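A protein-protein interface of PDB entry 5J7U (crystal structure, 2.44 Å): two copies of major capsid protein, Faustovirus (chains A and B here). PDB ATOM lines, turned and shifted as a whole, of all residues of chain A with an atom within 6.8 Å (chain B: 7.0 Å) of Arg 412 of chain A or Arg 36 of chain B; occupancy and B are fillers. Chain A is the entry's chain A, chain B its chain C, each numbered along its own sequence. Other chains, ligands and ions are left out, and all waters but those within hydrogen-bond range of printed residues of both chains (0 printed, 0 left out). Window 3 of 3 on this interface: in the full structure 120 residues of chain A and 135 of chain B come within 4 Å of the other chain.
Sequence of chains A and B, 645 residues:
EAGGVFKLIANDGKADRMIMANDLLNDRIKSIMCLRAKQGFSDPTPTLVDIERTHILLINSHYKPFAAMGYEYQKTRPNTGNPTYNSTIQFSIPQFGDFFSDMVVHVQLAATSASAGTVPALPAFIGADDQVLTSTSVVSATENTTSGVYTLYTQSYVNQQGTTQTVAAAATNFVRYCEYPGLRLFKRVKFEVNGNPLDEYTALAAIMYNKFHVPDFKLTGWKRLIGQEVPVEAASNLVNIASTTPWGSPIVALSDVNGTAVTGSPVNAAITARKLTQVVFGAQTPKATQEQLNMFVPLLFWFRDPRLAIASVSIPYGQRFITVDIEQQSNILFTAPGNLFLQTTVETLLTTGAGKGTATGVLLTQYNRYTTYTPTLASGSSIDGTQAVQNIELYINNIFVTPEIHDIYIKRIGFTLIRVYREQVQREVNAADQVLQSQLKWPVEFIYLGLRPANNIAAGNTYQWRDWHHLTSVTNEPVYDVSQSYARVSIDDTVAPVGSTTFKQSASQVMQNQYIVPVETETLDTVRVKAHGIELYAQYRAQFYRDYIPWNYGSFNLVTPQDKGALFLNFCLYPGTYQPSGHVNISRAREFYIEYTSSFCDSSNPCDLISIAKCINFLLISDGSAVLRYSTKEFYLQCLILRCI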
ATOM      1  N   ASP A 407     -25.870  28.164   8.619  1.00  0.00           N
ATOM      2  CA  ASP A 407     -26.557  28.960   7.609  1.00  0.00           C
ATOM      3  C   ASP A 407     -27.621  28.137   6.896  1.00  0.00           C
ATOM      4  O   ASP A 407     -28.736  28.619   6.659  1.00  0.00           O
ATOM      5  CB  ASP A 407     -25.546  29.519   6.611  1.00  0.00           C
ATOM      6  CG  ASP A 407     -26.165  30.502   5.643  1.00  0.00           C
ATOM      7  OD1 ASP A 407     -26.583  31.589   6.095  1.00  0.00           O
ATOM      8  OD2 ASP A 407     -26.227  30.195   4.434  1.00  0.00           O
ATOM      9  N   ILE A 408     -27.301  26.886   6.557  1.00  0.00           N
ATOM     10  CA  ILE A 408     -28.270  26.023   5.892  1.00  0.00           C
ATOM     11  C   ILE A 408     -29.431  25.699   6.823  1.00  0.00           C
ATOM     12  O   ILE A 408     -30.598  25.725   6.414  1.00  0.00           O
ATOM     13  CB  ILE A 408     -27.576  24.746   5.383  1.00  0.00           C
ATOM     14  CG1 ILE A 408     -26.556  25.095   4.302  1.00  0.00           C
ATOM     15  CG2 ILE A 408     -28.601  23.747   4.859  1.00  0.00           C
ATOM     16  CD1 ILE A 408     -25.624  23.959   3.957  1.00  0.00           C
ATOM     17  N   TYR A 409     -29.136  25.400   8.091  1.00  0.00           N
ATOM     18  CA  TYR A 409     -30.188  24.978   9.011  1.00  0.00           C
ATOM     19  C   TYR A 409     -31.164  26.109   9.304  1.00  0.00           C
ATOM     20  O   TYR A 409     -32.378  25.887   9.351  1.00  0.00           O
ATOM     21  CB  TYR A 409     -29.576  24.447  10.306  1.00  0.00           C
ATOM     22  CG  TYR A 409     -30.579  23.742  11.190  1.00  0.00           C
ATOM     23  CD1 TYR A 409     -31.097  22.506  10.829  1.00  0.00           C
ATOM     24  CD2 TYR A 409     -31.008  24.310  12.383  1.00  0.00           C
ATOM     25  CE1 TYR A 409     -32.017  21.857  11.628  1.00  0.00           C
ATOM     26  CE2 TYR A 409     -31.928  23.667  13.190  1.00  0.00           C
ATOM     27  CZ  TYR A 409     -32.428  22.440  12.807  1.00  0.00           C
ATOM     28  OH  TYR A 409     -33.343  21.792  13.605  1.00  0.00           O
ATOM     29  N   ILE A 410     -30.660  27.329   9.499  1.00  0.00           N
ATOM     30  CA  ILE A 410     -31.545  28.447   9.806  1.00  0.00           C
ATOM     31  C   ILE A 410     -32.402  28.810   8.596  1.00  0.00           C
ATOM     32  O   ILE A 410     -33.509  29.344   8.745  1.00  0.00           O
ATOM     33  CB  ILE A 410     -30.719  29.644  10.316  1.00  0.00           C
ATOM     34  CG1 ILE A 410     -29.993  29.263  11.605  1.00  0.00           C
ATOM     35  CG2 ILE A 410     -31.598  30.858  10.570  1.00  0.00           C
ATOM     36  CD1 ILE A 410     -30.914  28.736  12.679  1.00  0.00           C
ATOM     37  N   LYS A 411     -31.931  28.506   7.388  1.00  0.00           N
ATOM     38  CA  LYS A 411     -32.684  28.801   6.176  1.00  0.00           C
ATOM     39  C   LYS A 411     -33.625  27.679   5.755  1.00  0.00           C
ATOM     40  O   LYS A 411     -34.500  27.915   4.915  1.00  0.00           O
ATOM     41  CB  LYS A 411     -31.728  29.096   5.016  1.00  0.00           C
ATOM     42  CG  LYS A 411     -30.927  30.374   5.158  1.00  0.00           C
ATOM     43  CD  LYS A 411     -29.893  30.466   4.051  1.00  0.00           C
ATOM     44  CE  LYS A 411     -29.125  31.770   4.105  1.00  0.00           C
ATOM     45  NZ  LYS A 411     -28.158  31.870   2.976  1.00  0.00           N
ATOM     46  N   ARG A 412     -33.476  26.475   6.302  1.00  0.00           N
ATOM     47  CA  ARG A 412     -34.186  25.315   5.781  1.00  0.00           C
ATOM     48  C   ARG A 412     -35.161  24.671   6.752  1.00  0.00           C
ATOM     49  O   ARG A 412     -36.149  24.090   6.300  1.00  0.00           O
ATOM     50  CB  ARG A 412     -33.191  24.237   5.322  1.00  0.00           C
ATOM     51  CG  ARG A 412     -32.453  24.578   4.044  1.00  0.00           C
ATOM     52  CD  ARG A 412     -33.425  24.987   2.953  1.00  0.00           C
ATOM     53  NE  ARG A 412     -32.757  25.143   1.668  1.00  0.00           N
ATOM     54  CZ  ARG A 412     -33.318  25.688   0.594  1.00  0.00           C
ATOM     55  NH1 ARG A 412     -34.564  26.140   0.653  1.00  0.00           N
ATOM     56  NH2 ARG A 412     -32.630  25.787  -0.535  1.00  0.00           N
ATOM     57  N   ILE A 413     -34.917  24.744   8.061  1.00  0.00           N
ATOM     58  CA  ILE A 413     -35.705  23.942   8.992  1.00  0.00           C
ATOM     59  C   ILE A 413     -37.147  24.440   9.054  1.00  0.00           C
ATOM     60  O   ILE A 413     -38.087  23.643   9.164  1.00  0.00           O
ATOM     61  CB  ILE A 413     -35.033  23.918  10.378  1.00  0.00           C
ATOM     62  CG1 ILE A 413     -35.771  22.973  11.326  1.00  0.00           C
ATOM     63  CG2 ILE A 413     -34.945  25.301  10.952  1.00  0.00           C
ATOM     64  CD1 ILE A 413     -35.610  21.516  10.957  1.00  0.00           C
ATOM     65  N   GLY A 414     -37.352  25.752   8.963  1.00  0.00           N
ATOM     66  CA  GLY A 414     -38.693  26.302   8.975  1.00  0.00           C
ATOM     67  C   GLY A 414     -39.283  26.481  10.360  1.00  0.00           C
ATOM     68  O   GLY A 414     -39.607  27.602  10.761  1.00  0.00           O
ATOM     69  N   PHE A 415     -39.424  25.385  11.102  1.00  0.00           N
ATOM     70  CA  PHE A 415     -40.073  25.429  12.404  1.00  0.00           C
ATOM     71  C   PHE A 415     -39.640  24.215  13.214  1.00  0.00           C
ATOM     72  O   PHE A 415     -39.090  23.250  12.678  1.00  0.00           O
ATOM     73  CB  PHE A 415     -41.598  25.463  12.266  1.00  0.00           C
ATOM     74  CG  PHE A 415     -42.183  24.206  11.675  1.00  0.00           C
ATOM     75  CD1 PHE A 415     -42.140  23.982  10.309  1.00  0.00           C
ATOM     76  CD2 PHE A 415     -42.777  23.252  12.485  1.00  0.00           C
ATOM     77  CE1 PHE A 415     -42.675  22.827   9.762  1.00  0.00           C
ATOM     78  CE2 PHE A 415     -43.314  22.096  11.941  1.00  0.00           C
ATOM     79  CZ  PHE A 415     -43.264  21.888  10.576  1.00  0.00           C
ATOM     80  N   SER B  31     -20.001  22.540  -3.881  1.00  0.00           N
ATOM     81  CA  SER B  31     -20.424  21.982  -5.159  1.00  0.00           C
ATOM     82  C   SER B  31     -21.933  22.080  -5.345  1.00  0.00           C
ATOM     83  O   SER B  31     -22.405  22.349  -6.455  1.00  0.00           O
ATOM     84  CB  SER B  31     -19.966  20.529  -5.269  1.00  0.00           C
ATOM     85  OG  SER B  31     -20.686  19.836  -6.272  1.00  0.00           O
ATOM     86  N   ILE B  32     -22.706  21.865  -4.281  1.00  0.00           N
ATOM     87  CA  ILE B  32     -24.157  21.859  -4.442  1.00  0.00           C
ATOM     88  C   ILE B  32     -24.677  23.275  -4.670  1.00  0.00           C
ATOM     89  O   ILE B  32     -25.572  23.487  -5.494  1.00  0.00           O
ATOM     90  CB  ILE B  32     -24.840  21.167  -3.246  1.00  0.00           C
ATOM     91  CG1 ILE B  32     -26.318  20.912  -3.539  1.00  0.00           C
ATOM     92  CG2 ILE B  32     -24.712  21.980  -1.998  1.00  0.00           C
ATOM     93  CD1 ILE B  32     -26.553  19.860  -4.593  1.00  0.00           C
ATOM     94  N   MET B  33     -24.107  24.269  -3.980  1.00  0.00           N
ATOM     95  CA  MET B  33     -24.483  25.654  -4.256  1.00  0.00           C
ATOM     96  C   MET B  33     -24.105  26.044  -5.677  1.00  0.00           C
ATOM     97  O   MET B  33     -24.828  26.800  -6.336  1.00  0.00           O
ATOM     98  CB  MET B  33     -23.817  26.604  -3.259  1.00  0.00           C
ATOM     99  CG  MET B  33     -24.266  26.449  -1.819  1.00  0.00           C
ATOM    100  SD  MET B  33     -23.547  27.721  -0.761  1.00  0.00           S
ATOM    101  CE  MET B  33     -24.559  29.135  -1.186  1.00  0.00           C
ATOM    102  N   CYS B  34     -22.970  25.536  -6.162  1.00  0.00           N
ATOM    103  CA  CYS B  34     -22.534  25.852  -7.517  1.00  0.00           C
ATOM    104  C   CYS B  34     -23.521  25.331  -8.555  1.00  0.00           C
ATOM    105  O   CYS B  34     -23.767  25.988  -9.573  1.00  0.00           O
ATOM    106  CB  CYS B  34     -21.141  25.271  -7.762  1.00  0.00           C
ATOM    107  SG  CYS B  34     -20.529  25.501  -9.443  1.00  0.00           S
ATOM    108  N   LEU B  35     -24.101  24.153  -8.312  1.00  0.00           N
ATOM    109  CA  LEU B  35     -25.024  23.568  -9.277  1.00  0.00           C
ATOM    110  C   LEU B  35     -26.401  24.214  -9.194  1.00  0.00           C
ATOM    111  O   LEU B  35     -27.004  24.533 -10.222  1.00  0.00           O
ATOM    112  CB  LEU B  35     -25.128  22.057  -9.061  1.00  0.00           C
ATOM    113  CG  LEU B  35     -23.825  21.285  -9.257  1.00  0.00           C
ATOM    114  CD1 LEU B  35     -24.097  19.803  -9.452  1.00  0.00           C
ATOM    115  CD2 LEU B  35     -23.057  21.849 -10.436  1.00  0.00           C
ATOM    116  N   ARG B  36     -26.912  24.406  -7.973  1.00  0.00           N
ATOM    117  CA  ARG B  36     -28.177  25.114  -7.801  1.00  0.00           C
ATOM    118  C   ARG B  36     -28.154  26.453  -8.526  1.00  0.00           C
ATOM    119  O   ARG B  36     -29.112  26.808  -9.223  1.00  0.00           O
ATOM    120  CB  ARG B  36     -28.466  25.315  -6.312  1.00  0.00           C
ATOM    121  CG  ARG B  36     -28.509  24.034  -5.493  1.00  0.00           C
ATOM    122  CD  ARG B  36     -29.924  23.602  -5.209  1.00  0.00           C
ATOM    123  NE  ARG B  36     -30.705  24.710  -4.677  1.00  0.00           N
ATOM    124  CZ  ARG B  36     -32.011  24.661  -4.449  1.00  0.00           C
ATOM    125  NH1 ARG B  36     -32.688  23.550  -4.703  1.00  0.00           N
ATOM    126  NH2 ARG B  36     -32.639  25.722  -3.967  1.00  0.00           N
ATOM    127  N   ALA B  37     -27.061  27.202  -8.387  1.00  0.00           N
ATOM    128  CA  ALA B  37     -26.926  28.462  -9.113  1.00  0.00           C
ATOM    129  C   ALA B  37     -26.909  28.227 -10.619  1.00  0.00           C
ATOM    130  O   ALA B  37     -27.656  28.865 -11.369  1.00  0.00           O
ATOM    131  CB  ALA B  37     -25.659  29.192  -8.668  1.00  0.00           C
ATOM    132  N   LYS B  38     -26.065  27.297 -11.075  1.00  0.00           N
ATOM    133  CA  LYS B  38     -25.894  27.064 -12.506  1.00  0.00           C
ATOM    134  C   LYS B  38     -27.207  26.683 -13.182  1.00  0.00           C
ATOM    135  O   LYS B  38     -27.472  27.096 -14.317  1.00  0.00           O
ATOM    136  CB  LYS B  38     -24.839  25.977 -12.724  1.00  0.00           C
ATOM    137  CG  LYS B  38     -24.760  25.430 -14.140  1.00  0.00           C
ATOM    138  CD  LYS B  38     -23.490  24.621 -14.336  1.00  0.00           C
ATOM    139  CE  LYS B  38     -22.264  25.467 -14.025  1.00  0.00           C
ATOM    140  NZ  LYS B  38     -20.989  24.761 -14.320  1.00  0.00           N
ATOM    141  N   GLN B  39     -28.047  25.913 -12.495  1.00  0.00           N
ATOM    142  CA  GLN B  39     -29.265  25.377 -13.090  1.00  0.00           C
ATOM    143  C   GLN B  39     -30.434  26.353 -13.073  1.00  0.00           C
ATOM    144  O   GLN B  39     -31.510  26.005 -13.573  1.00  0.00           O
ATOM    145  CB  GLN B  39     -29.665  24.086 -12.375  1.00  0.00           C
ATOM    146  CG  GLN B  39     -28.619  22.995 -12.462  1.00  0.00           C
ATOM    147  CD  GLN B  39     -28.987  21.780 -11.646  1.00  0.00           C
ATOM    148  OE1 GLN B  39     -30.018  21.760 -10.978  1.00  0.00           O
ATOM    149  NE2 GLN B  39     -28.143  20.756 -11.695  1.00  0.00           N
ATOM    150  N   GLY B  40     -30.260  27.547 -12.514  1.00  0.00           N
ATOM    151  CA  GLY B  40     -31.323  28.530 -12.493  1.00  0.00           C
ATOM    152  C   GLY B  40     -32.181  28.543 -11.250  1.00  0.00           C
ATOM    153  O   GLY B  40     -33.310  29.040 -11.303  1.00  0.00           O
ATOM    154  N   PHE B  41     -31.690  28.011 -10.134  1.00  0.00           N
ATOM    155  CA  PHE B  41     -32.440  28.062  -8.890  1.00  0.00           C
ATOM    156  C   PHE B  41     -32.354  29.452  -8.274  1.00  0.00           C
ATOM    157  O   PHE B  41     -31.346  30.153  -8.395  1.00  0.00           O
ATOM    158  CB  PHE B  41     -31.927  27.018  -7.899  1.00  0.00           C
ATOM    159  CG  PHE B  41     -32.389  25.622  -8.198  1.00  0.00           C
ATOM    160  CD1 PHE B  41     -33.654  25.205  -7.819  1.00  0.00           C
ATOM    161  CD2 PHE B  41     -31.561  24.725  -8.853  1.00  0.00           C
ATOM    162  CE1 PHE B  41     -34.088  23.922  -8.088  1.00  0.00           C
ATOM    163  CE2 PHE B  41     -31.989  23.438  -9.124  1.00  0.00           C
ATOM    164  CZ  PHE B  41     -33.255  23.036  -8.742  1.00  0.00           C
ATOM    165  N   SER B  42     -33.440  29.846  -7.607  1.00  0.00           N
ATOM    166  CA  SER B  42     -33.487  31.159  -6.974  1.00  0.00           C
ATOM    167  C   SER B  42     -32.576  31.212  -5.751  1.00  0.00           C
ATOM    168  O   SER B  42     -31.829  32.181  -5.565  1.00  0.00           O
ATOM    169  CB  SER B  42     -34.929  31.492  -6.596  1.00  0.00           C
ATOM    170  OG  SER B  42     -35.055  32.842  -6.190  1.00  0.00           O
ATOM    171  N   ASP B  43     -32.626  30.179  -4.917  1.00  0.00           N
ATOM    172  CA  ASP B  43     -31.857  30.102  -3.679  1.00  0.00           C
ATOM    173  C   ASP B  43     -30.773  29.044  -3.832  1.00  0.00           C
ATOM    174  O   ASP B  43     -31.094  27.847  -3.899  1.00  0.00           O
ATOM    175  CB  ASP B  43     -32.788  29.757  -2.513  1.00  0.00           C
ATOM    176  CG  ASP B  43     -32.096  29.798  -1.161  1.00  0.00           C
ATOM    177  OD1 ASP B  43     -30.866  30.004  -1.103  1.00  0.00           O
ATOM    178  OD2 ASP B  43     -32.798  29.609  -0.145  1.00  0.00           O
ATOM    179  N   PRO B  44     -29.490  29.417  -3.885  1.00  0.00           N
ATOM    180  CA  PRO B  44     -28.441  28.405  -4.094  1.00  0.00           C
ATOM    181  C   PRO B  44     -28.188  27.525  -2.885  1.00  0.00           C
ATOM    182  O   PRO B  44     -27.544  26.477  -3.033  1.00  0.00           O
ATOM    183  CB  PRO B  44     -27.196  29.245  -4.426  1.00  0.00           C
ATOM    184  CG  PRO B  44     -27.679  30.666  -4.577  1.00  0.00           C
ATOM    185  CD  PRO B  44     -28.927  30.769  -3.765  1.00  0.00           C
ATOM    186  N   THR B  45     -28.669  27.904  -1.704  1.00  0.00           N
ATOM    187  CA  THR B  45     -28.301  27.188  -0.493  1.00  0.00           C
ATOM    188  C   THR B  45     -28.916  25.788  -0.487  1.00  0.00           C
ATOM    189  O   THR B  45     -30.054  25.603  -0.933  1.00  0.00           O
ATOM    190  CB  THR B  45     -28.735  27.965   0.750  1.00  0.00           C
ATOM    191  OG1 THR B  45     -30.145  28.207   0.703  1.00  0.00           O
ATOM    192  CG2 THR B  45     -27.993  29.296   0.825  1.00  0.00           C
ATOM    193  N   PRO B  46     -28.192  24.792   0.013  1.00  0.00           N
ATOM    194  CA  PRO B  46     -28.647  23.401  -0.098  1.00  0.00           C
ATOM    195  C   PRO B  46     -29.888  23.136   0.741  1.00  0.00           C
ATOM    196  O   PRO B  46     -30.310  23.942   1.573  1.00  0.00           O
ATOM    197  CB  PRO B  46     -27.456  22.589   0.421  1.00  0.00           C
ATOM    198  CG  PRO B  46     -26.308  23.551   0.495  1.00  0.00           C
ATOM    199  CD  PRO B  46     -26.876  24.907   0.659  1.00  0.00           C
ATOM    200  N   THR B  47     -30.471  21.965   0.505  1.00  0.00           N
ATOM    201  CA  THR B  47     -31.577  21.466   1.305  1.00  0.00           C
ATOM    202  C   THR B  47     -31.039  20.593   2.434  1.00  0.00           C
ATOM    203  O   THR B  47     -29.903  20.116   2.394  1.00  0.00           O
ATOM    204  CB  THR B  47     -32.554  20.662   0.445  1.00  0.00           C
ATOM    205  OG1 THR B  47     -32.053  19.332   0.264  1.00  0.00           O
ATOM    206  CG2 THR B  47     -32.728  21.319  -0.921  1.00  0.00           C
ATOM    207  N   LEU B  48     -31.875  20.387   3.454  1.00  0.00           N
ATOM    208  CA  LEU B  48     -31.438  19.580   4.589  1.00  0.00           C
ATOM    209  C   LEU B  48     -31.236  18.121   4.201  1.00  0.00           C
ATOM    210  O   LEU B  48     -30.379  17.446   4.782  1.00  0.00           O
ATOM    211  CB  LEU B  48     -32.434  19.693   5.744  1.00  0.00           C
ATOM    212  CG  LEU B  48     -32.325  20.972   6.580  1.00  0.00           C
ATOM    213  CD1 LEU B  48     -33.149  20.870   7.854  1.00  0.00           C
ATOM    214  CD2 LEU B  48     -30.871  21.282   6.902  1.00  0.00           C
ATOM    215  N   ASP B  50     -30.165  17.203   1.215  1.00  0.00           N
ATOM    216  CA  ASP B  50     -28.888  17.219   0.509  1.00  0.00           C
ATOM    217  C   ASP B  50     -27.744  16.907   1.463  1.00  0.00           C
ATOM    218  O   ASP B  50     -26.913  16.031   1.199  1.00  0.00           O
ATOM    219  CB  ASP B  50     -28.665  18.577  -0.160  1.00  0.00           C
ATOM    220  CG  ASP B  50     -29.413  18.717  -1.470  1.00  0.00           C
ATOM    221  OD1 ASP B  50     -29.865  17.687  -2.011  1.00  0.00           O
ATOM    222  OD2 ASP B  50     -29.535  19.860  -1.964  1.00  0.00           O
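Printed residues of chain B within 4 Å of Ile 408 of chain A: Pro 46 and Leu 48.
Printed residues of chain B within 4 Å of Arg 412 of chain A: Arg 36 (3.4 Å), Asp 43 (3.8 Å), Thr 45 (2.6 Å), Pro 46 (2.7 Å), Thr 47 (3.9 Å) and Leu 48 (3.6 Å).
Arg 36 of chain B touches just one residue of chain A: Arg 412 (3.4 Å).
Of the printed residues of chain A, Asp 43 of chain B touches Arg 412 (3.8 Å).
Of the printed residues of chain A, Thr 45 of chain B touches Lys 411 (3.4 Å) and Arg 412 (2.6 Å).
Of the printed residues of chain A, Thr 47 of chain B touches Arg 412.
Of the printed residues of chain A, Leu 48 of chain B touches Ile 408, Tyr 409 and Arg 412.
The nearest residue of chain B that does not touch Arg 412 of chain A is Pro 44 of chain B (5.3 Å).
The nearest printed residue of chain A that does not touch Arg 36 of chain B is Lys 411 of chain A (9.3 Å).
Among the printed residues, merely in contact across the chains: Ile 408 of chain A with Pro 46 of chain B (3.6 Å), Ile 408 of chain A with Leu 48 of chain B (3.9 Å), Tyr 409 of chain A with Leu 48 of chain B (3.97 Å), Lys 411 of chain A with Thr 45 of chain B (3.4 Å), Arg 412 of chain A with Thr 47 of chain B (3.9 Å) and Arg 412 of chain A with Leu 48 of chain B (3.6 Å).
No position is printed for both chains.
Of the 10 pairs that touch across the chains among the printed residues, none has its exchanged pair printed and touching as well.
Of the 19 printed residues of chain B, 6 touch a printed residue of chain A.
Among the printed residues, Asp or Glu carboxylates within 4 Å of a Lys or Arg side-chain nitrogen of the other chain: Arg 412 of chain A with Asp 43 of chain B (3.8 Å).
The guanidinium group (NH2) of Arg 412 of chain A is in salt-bridge range of the side-chain carboxylate (OD2) of Asp 43 of chain B, at 3.8 Å.
NH2 of Arg 412 of chain A sits at hydrogen-bond distance from O of Thr 45 of chain B, at 2.6 Å.
The guanidinium group (NE) of Arg 412 of chain A is in hydrogen-bond range of the backbone carbonyl oxygen (O) of Pro 46 of chain B (2.7 Å).
The guanidinium group (NH2) of Arg 412 of chain A sits close to the guanidinium group (NH2) of Arg 36 of chain B, at 3.4 Å.
OD2 of Asp 407 of chain A is in salt-bridge range of NZ of Lys 411 of chain A.
O of Arg 36 of chain B is in hydrogen-bond range of N of Phe 41 of chain B (3.0 Å).
NH2 of Arg 36 of chain B sits at hydrogen-bond distance from O of Asp 43 of chain B, 2.6 Å away.
The side-chain hydroxyl of Thr 45 of chain B is in hydrogen-bond range of the side-chain carboxylate of Asp 43 of chain B (2.6 Å).
The backbone NH (N) of Asp 50 of chain B lies within hydrogen-bond range of the side-chain hydroxyl (OG1) of Thr 47 of chain B, at 3.0 Å.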
